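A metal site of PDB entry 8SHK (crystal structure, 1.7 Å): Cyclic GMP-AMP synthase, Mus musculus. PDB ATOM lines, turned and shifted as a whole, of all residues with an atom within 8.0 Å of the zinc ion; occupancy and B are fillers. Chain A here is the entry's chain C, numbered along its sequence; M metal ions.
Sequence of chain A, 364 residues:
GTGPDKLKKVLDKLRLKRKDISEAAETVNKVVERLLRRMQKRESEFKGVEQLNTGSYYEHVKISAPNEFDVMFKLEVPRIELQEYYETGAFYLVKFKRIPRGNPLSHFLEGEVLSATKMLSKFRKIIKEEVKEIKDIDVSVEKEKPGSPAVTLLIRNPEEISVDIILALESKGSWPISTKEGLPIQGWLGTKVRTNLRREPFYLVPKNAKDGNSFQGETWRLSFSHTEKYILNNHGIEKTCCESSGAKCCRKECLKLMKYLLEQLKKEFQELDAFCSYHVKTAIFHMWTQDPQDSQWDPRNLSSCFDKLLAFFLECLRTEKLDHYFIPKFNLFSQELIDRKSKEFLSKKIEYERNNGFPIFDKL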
ATOM      1  N   LEU A 232     -18.593 -18.571  11.407  1.00  0.00           N
ATOM      2  CA  LEU A 232     -19.763 -17.758  11.067  1.00  0.00           C
ATOM      3  C   LEU A 232     -19.394 -16.642  10.100  1.00  0.00           C
ATOM      4  O   LEU A 232     -20.188 -16.295   9.215  1.00  0.00           O
ATOM      5  CB  LEU A 232     -20.417 -17.157  12.322  1.00  0.00           C
ATOM      6  CG  LEU A 232     -21.554 -17.953  12.937  1.00  0.00           C
ATOM      7  CD1 LEU A 232     -22.813 -17.809  12.058  1.00  0.00           C
ATOM      8  CD2 LEU A 232     -21.210 -19.406  13.097  1.00  0.00           C
ATOM      9  N   ASN A 233     -18.226 -16.032  10.280  1.00  0.00           N
ATOM     10  CA  ASN A 233     -17.870 -14.883   9.459  1.00  0.00           C
ATOM     11  C   ASN A 233     -17.054 -15.259   8.223  1.00  0.00           C
ATOM     12  O   ASN A 233     -16.723 -14.387   7.422  1.00  0.00           O
ATOM     13  CB  ASN A 233     -17.121 -13.847  10.311  1.00  0.00           C
ATOM     14  CG  ASN A 233     -18.041 -13.216  11.373  1.00  0.00           C
ATOM     15  OD1 ASN A 233     -19.269 -13.253  11.247  1.00  0.00           O
ATOM     16  ND2 ASN A 233     -17.443 -12.621  12.403  1.00  0.00           N
ATOM     17  N   ASN A 234     -16.732 -16.555   8.055  1.00  0.00           N
ATOM     18  CA  ASN A 234     -15.987 -17.067   6.909  1.00  0.00           C
ATOM     19  C   ASN A 234     -16.624 -18.407   6.521  1.00  0.00           C
ATOM     20  O   ASN A 234     -16.025 -19.473   6.596  1.00  0.00           O
ATOM     21  CB  ASN A 234     -14.510 -17.253   7.228  1.00  0.00           C
ATOM     22  CG  ASN A 234     -13.830 -15.969   7.654  1.00  0.00           C
ATOM     23  OD1 ASN A 234     -13.226 -15.294   6.832  1.00  0.00           O
ATOM     24  ND2 ASN A 234     -13.918 -15.622   8.950  1.00  0.00           N
ATOM     25  N   HIS A 235     -17.891 -18.361   6.106  1.00  0.00           N
ATOM     26  CA  HIS A 235     -18.752 -19.535   6.095  1.00  0.00           C
ATOM     27  C   HIS A 235     -18.960 -20.134   4.697  1.00  0.00           C
ATOM     28  O   HIS A 235     -19.692 -21.115   4.583  1.00  0.00           O
ATOM     29  CB  HIS A 235     -20.114 -19.166   6.670  1.00  0.00           C
ATOM     30  CG  HIS A 235     -20.758 -18.028   5.943  1.00  0.00           C
ATOM     31  ND1 HIS A 235     -21.016 -16.812   6.538  1.00  0.00           N
ATOM     32  CD2 HIS A 235     -21.144 -17.913   4.647  1.00  0.00           C
ATOM     33  CE1 HIS A 235     -21.573 -16.004   5.625  1.00  0.00           C
ATOM     34  NE2 HIS A 235     -21.627 -16.637   4.473  1.00  0.00           N
ATOM     35  N   GLY A 236     -18.360 -19.566   3.662  1.00  0.00           N
ATOM     36  CA  GLY A 236     -18.613 -20.017   2.305  1.00  0.00           C
ATOM     37  C   GLY A 236     -17.536 -20.950   1.790  1.00  0.00           C
ATOM     38  O   GLY A 236     -16.408 -20.966   2.267  1.00  0.00           O
ATOM     39  N   ILE A 237     -17.895 -21.766   0.802  1.00  0.00           N
ATOM     40  CA  ILE A 237     -16.843 -22.487   0.103  1.00  0.00           C
ATOM     41  C   ILE A 237     -16.057 -21.513  -0.754  1.00  0.00           C
ATOM     42  O   ILE A 237     -14.836 -21.657  -0.921  1.00  0.00           O
ATOM     43  CB  ILE A 237     -17.431 -23.660  -0.701  1.00  0.00           C
ATOM     44  CG1 ILE A 237     -16.339 -24.642  -1.118  1.00  0.00           C
ATOM     45  CG2 ILE A 237     -18.220 -23.147  -1.898  1.00  0.00           C
ATOM     46  CD1 ILE A 237     -16.923 -25.973  -1.566  1.00  0.00           C
ATOM     47  N   GLU A 238     -16.700 -20.464  -1.254  1.00  0.00           N
ATOM     48  CA  GLU A 238     -15.977 -19.418  -1.952  1.00  0.00           C
ATOM     49  C   GLU A 238     -15.541 -18.359  -0.947  1.00  0.00           C
ATOM     50  O   GLU A 238     -16.291 -17.999  -0.025  1.00  0.00           O
ATOM     51  CB  GLU A 238     -16.852 -18.768  -3.019  1.00  0.00           C
ATOM     52  CG  GLU A 238     -17.111 -19.703  -4.209  1.00  0.00           C
ATOM     53  CD  GLU A 238     -17.670 -18.990  -5.406  1.00  0.00           C
ATOM     54  OE1 GLU A 238     -17.955 -19.651  -6.415  1.00  0.00           O
ATOM     55  OE2 GLU A 238     -17.766 -17.758  -5.360  1.00  0.00           O
ATOM     56  N   THR A 240     -15.203 -15.306  -1.320  1.00  0.00           N
ATOM     57  CA  THR A 240     -15.934 -14.067  -1.480  1.00  0.00           C
ATOM     58  C   THR A 240     -17.399 -14.164  -1.076  1.00  0.00           C
ATOM     59  O   THR A 240     -18.138 -13.193  -1.272  1.00  0.00           O
ATOM     60  CB  THR A 240     -15.840 -13.583  -2.929  1.00  0.00           C
ATOM     61  OG1 THR A 240     -16.344 -14.595  -3.802  1.00  0.00           O
ATOM     62  CG2 THR A 240     -14.384 -13.287  -3.301  1.00  0.00           C
ATOM     63  N   CYS A 241     -17.843 -15.294  -0.522  1.00  0.00           N
ATOM     64  CA  CYS A 241     -19.227 -15.448  -0.084  1.00  0.00           C
ATOM     65  C   CYS A 241     -19.626 -14.326   0.883  1.00  0.00           C
ATOM     66  O   CYS A 241     -18.952 -14.088   1.893  1.00  0.00           O
ATOM     67  CB  CYS A 241     -19.427 -16.819   0.593  1.00  0.00           C
ATOM     68  SG  CYS A 241     -21.167 -17.295   0.923  1.00  0.00           S
ATOM     69  N   CYS A 242     -20.692 -13.611   0.518  1.00  0.00           N
ATOM     70  CA  CYS A 242     -21.239 -12.481   1.270  1.00  0.00           C
ATOM     71  C   CYS A 242     -20.286 -11.285   1.345  1.00  0.00           C
ATOM     72  O   CYS A 242     -20.502 -10.369   2.154  1.00  0.00           O
ATOM     73  CB  CYS A 242     -21.698 -12.896   2.670  1.00  0.00           C
ATOM     74  SG  CYS A 242     -23.130 -14.048   2.700  1.00  0.00           S
ATOM     75  N   GLU A 243     -19.256 -11.233   0.509  1.00  0.00           N
ATOM     76  CA  GLU A 243     -18.434 -10.027   0.435  1.00  0.00           C
ATOM     77  C   GLU A 243     -18.927  -9.107  -0.673  1.00  0.00           C
ATOM     78  O   GLU A 243     -19.745  -9.473  -1.523  1.00  0.00           O
ATOM     79  CB  GLU A 243     -16.959 -10.360   0.182  1.00  0.00           C
ATOM     80  CG  GLU A 243     -16.252 -11.111   1.326  1.00  0.00           C
ATOM     81  CD  GLU A 243     -14.775 -11.291   1.031  1.00  0.00           C
ATOM     82  OE1 GLU A 243     -14.363 -11.061  -0.123  1.00  0.00           O
ATOM     83  OE2 GLU A 243     -14.012 -11.643   1.956  1.00  0.00           O
ATOM     84  N   ALA A 247     -21.039 -13.119  -3.806  1.00  0.00           N
ATOM     85  CA  ALA A 247     -22.460 -13.399  -3.853  1.00  0.00           C
ATOM     86  C   ALA A 247     -22.992 -13.636  -2.453  1.00  0.00           C
ATOM     87  O   ALA A 247     -22.342 -14.304  -1.650  1.00  0.00           O
ATOM     88  CB  ALA A 247     -22.747 -14.622  -4.737  1.00  0.00           C
ATOM     89  N   LYS A 248     -24.153 -13.073  -2.145  1.00  0.00           N
ATOM     90  CA  LYS A 248     -24.805 -13.368  -0.881  1.00  0.00           C
ATOM     91  C   LYS A 248     -25.284 -14.806  -0.846  1.00  0.00           C
ATOM     92  O   LYS A 248     -25.712 -15.352  -1.871  1.00  0.00           O
ATOM     93  CB  LYS A 248     -25.990 -12.424  -0.655  1.00  0.00           C
ATOM     94  CG  LYS A 248     -25.625 -11.094  -0.043  1.00  0.00           C
ATOM     95  CD  LYS A 248     -25.339 -11.247   1.438  1.00  0.00           C
ATOM     96  CE  LYS A 248     -26.613 -11.585   2.208  1.00  0.00           C
ATOM     97  NZ  LYS A 248     -26.395 -12.572   3.309  1.00  0.00           N
ATOM     98  N   CYS A 249     -25.238 -15.425   0.336  1.00  0.00           N
ATOM     99  CA  CYS A 249     -25.928 -16.685   0.627  1.00  0.00           C
ATOM    100  C   CYS A 249     -26.925 -16.444   1.763  1.00  0.00           C
ATOM    101  O   CYS A 249     -26.995 -15.358   2.316  1.00  0.00           O
ATOM    102  CB  CYS A 249     -24.938 -17.783   1.022  1.00  0.00           C
ATOM    103  SG  CYS A 249     -24.284 -17.609   2.734  1.00  0.00           S
ATOM    104  N   CYS A 250     -27.723 -17.469   2.088  1.00  0.00           N
ATOM    105  CA  CYS A 250     -28.700 -17.334   3.163  1.00  0.00           C
ATOM    106  C   CYS A 250     -28.339 -18.162   4.400  1.00  0.00           C
ATOM    107  O   CYS A 250     -29.223 -18.457   5.214  1.00  0.00           O
ATOM    108  CB  CYS A 250     -30.112 -17.689   2.695  1.00  0.00           C
ATOM    109  SG  CYS A 250     -30.347 -19.434   2.252  1.00  0.00           S
ATOM    110  N   ARG A 251     -27.059 -18.501   4.584  1.00  0.00           N
ATOM    111  CA  ARG A 251     -26.646 -19.327   5.712  1.00  0.00           C
ATOM    112  C   ARG A 251     -26.966 -18.652   7.058  1.00  0.00           C
ATOM    113  O   ARG A 251     -27.598 -19.269   7.923  1.00  0.00           O
ATOM    114  CB  ARG A 251     -25.149 -19.626   5.615  1.00  0.00           C
ATOM    115  CG  ARG A 251     -24.804 -20.727   4.592  1.00  0.00           C
ATOM    116  CD  ARG A 251     -23.323 -21.102   4.706  1.00  0.00           C
ATOM    117  NE  ARG A 251     -22.891 -22.073   3.702  1.00  0.00           N
ATOM    118  CZ  ARG A 251     -22.325 -21.737   2.547  1.00  0.00           C
ATOM    119  NH1 ARG A 251     -22.313 -20.474   2.124  1.00  0.00           N
ATOM    120  NH2 ARG A 251     -21.752 -22.681   1.804  1.00  0.00           N
ATOM    121  N   LYS A 252     -26.531 -17.402   7.242  1.00  0.00           N
ATOM    122  CA  LYS A 252     -26.768 -16.743   8.526  1.00  0.00           C
ATOM    123  C   LYS A 252     -28.237 -16.414   8.724  1.00  0.00           C
ATOM    124  O   LYS A 252     -28.738 -16.431   9.851  1.00  0.00           O
ATOM    125  CB  LYS A 252     -25.923 -15.458   8.633  1.00  0.00           C
ATOM    126  CG  LYS A 252     -24.410 -15.697   8.568  1.00  0.00           C
ATOM    127  CD  LYS A 252     -23.599 -14.415   8.836  1.00  0.00           C
ATOM    128  CE  LYS A 252     -22.844 -14.486  10.150  1.00  0.00           C
ATOM    129  NZ  LYS A 252     -21.814 -13.394  10.213  1.00  0.00           N
ATOM    130  N   GLU A 253     -28.937 -16.083   7.636  1.00  0.00           N
ATOM    131  CA  GLU A 253     -30.376 -15.831   7.729  1.00  0.00           C
ATOM    132  C   GLU A 253     -31.116 -17.057   8.262  1.00  0.00           C
ATOM    133  O   GLU A 253     -32.051 -16.941   9.057  1.00  0.00           O
ATOM    134  CB  GLU A 253     -30.894 -15.417   6.360  1.00  0.00           C
ATOM    135  CG  GLU A 253     -30.474 -14.023   5.895  1.00  0.00           C
ATOM    136  CD  GLU A 253     -29.012 -13.909   5.461  1.00  0.00           C
ATOM    137  OE1 GLU A 253     -28.521 -12.756   5.380  1.00  0.00           O
ATOM    138  OE2 GLU A 253     -28.313 -14.931   5.308  1.00  0.00           O
ATOM    139  N   ASP A 294     -21.991 -23.140  -1.754  1.00  0.00           N
ATOM    140  CA  ASP A 294     -22.683 -21.858  -1.628  1.00  0.00           C
ATOM    141  C   ASP A 294     -23.981 -21.854  -2.442  1.00  0.00           C
ATOM    142  O   ASP A 294     -24.961 -21.229  -2.035  1.00  0.00           O
ATOM    143  CB  ASP A 294     -21.792 -20.693  -2.063  1.00  0.00           C
ATOM    144  CG  ASP A 294     -20.548 -20.551  -1.202  1.00  0.00           C
ATOM    145  OD1 ASP A 294     -20.517 -21.143  -0.109  1.00  0.00           O
ATOM    146  OD2 ASP A 294     -19.617 -19.833  -1.624  1.00  0.00           O
ATOM    147  N   TRP A 297     -27.140 -22.646  -0.781  1.00  0.00           N
ATOM    148  CA  TRP A 297     -27.642 -21.640   0.149  1.00  0.00           C
ATOM    149  C   TRP A 297     -27.888 -20.326  -0.575  1.00  0.00           C
ATOM    150  O   TRP A 297     -27.639 -19.236  -0.040  1.00  0.00           O
ATOM    151  CB  TRP A 297     -26.672 -21.477   1.330  1.00  0.00           C
ATOM    152  CG  TRP A 297     -26.518 -22.762   2.078  1.00  0.00           C
ATOM    153  CD1 TRP A 297     -25.666 -23.788   1.776  1.00  0.00           C
ATOM    154  CD2 TRP A 297     -27.270 -23.192   3.229  1.00  0.00           C
ATOM    155  NE1 TRP A 297     -25.818 -24.819   2.673  1.00  0.00           N
ATOM    156  CE2 TRP A 297     -26.802 -24.486   3.567  1.00  0.00           C
ATOM    157  CE3 TRP A 297     -28.281 -22.608   4.008  1.00  0.00           C
ATOM    158  CZ2 TRP A 297     -27.310 -25.209   4.659  1.00  0.00           C
ATOM    159  CZ3 TRP A 297     -28.801 -23.336   5.085  1.00  0.00           C
ATOM    160  CH2 TRP A 297     -28.283 -24.618   5.405  1.00  0.00           C
ATOM    161  N   PRO A 299     -29.821 -17.132  -1.820  1.00  0.00           N
ATOM    162  CA  PRO A 299     -30.902 -16.381  -1.148  1.00  0.00           C
ATOM    163  C   PRO A 299     -32.288 -16.735  -1.663  1.00  0.00           C
ATOM    164  O   PRO A 299     -33.251 -16.723  -0.890  1.00  0.00           O
ATOM    165  CB  PRO A 299     -30.548 -14.926  -1.460  1.00  0.00           C
ATOM    166  CG  PRO A 299     -29.051 -14.943  -1.559  1.00  0.00           C
ATOM    167  CD  PRO A 299     -28.768 -16.231  -2.310  1.00  0.00           C
HETATM  168 ZN    ZN M   1     -22.381 -16.220   2.603  1.00  0.00          ZN
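The backbone carbonyl oxygen (O) of His 235 sits close to the guanidinium group (NE) of Arg 251. The backbone carbonyl oxygen of Leu 232 lies within hydrogen-bond range of a ring nitrogen (ND1) of His 235, at 2.8 Å. The backbone carbonyl oxygen (O) of Ala 247 lies within hydrogen-bond range of the backbone NH (N) of Cys 242 (2.8 Å). The side-chain amino group (NZ) of Lys 248 lies close to the side-chain sulfur (SG) of Cys 242 (3.6 Å). The guanidinium group of Arg 251 sits close to the side-chain sulfur of Cys 241 (3.6 Å). The backbone NH (N) of Arg 251 lies close to the side-chain sulfur (SG) of Cys 249 (3.5 Å).
Of the 21 residues printed, 4 come within 4 Å of the zinc ion. The nearest printed residue that does not touch the zinc ion is Arg 251 (4.3 Å).
The zinc ion is bound by a ring nitrogen (NE2) of His 235 (2.1 Å), the side-chain sulfur of Cys 242 (2.3 Å), the side-chain sulfur of Cys 241 (2.3 Å) and the side-chain sulfur of Cys 249 (2.4 Å).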
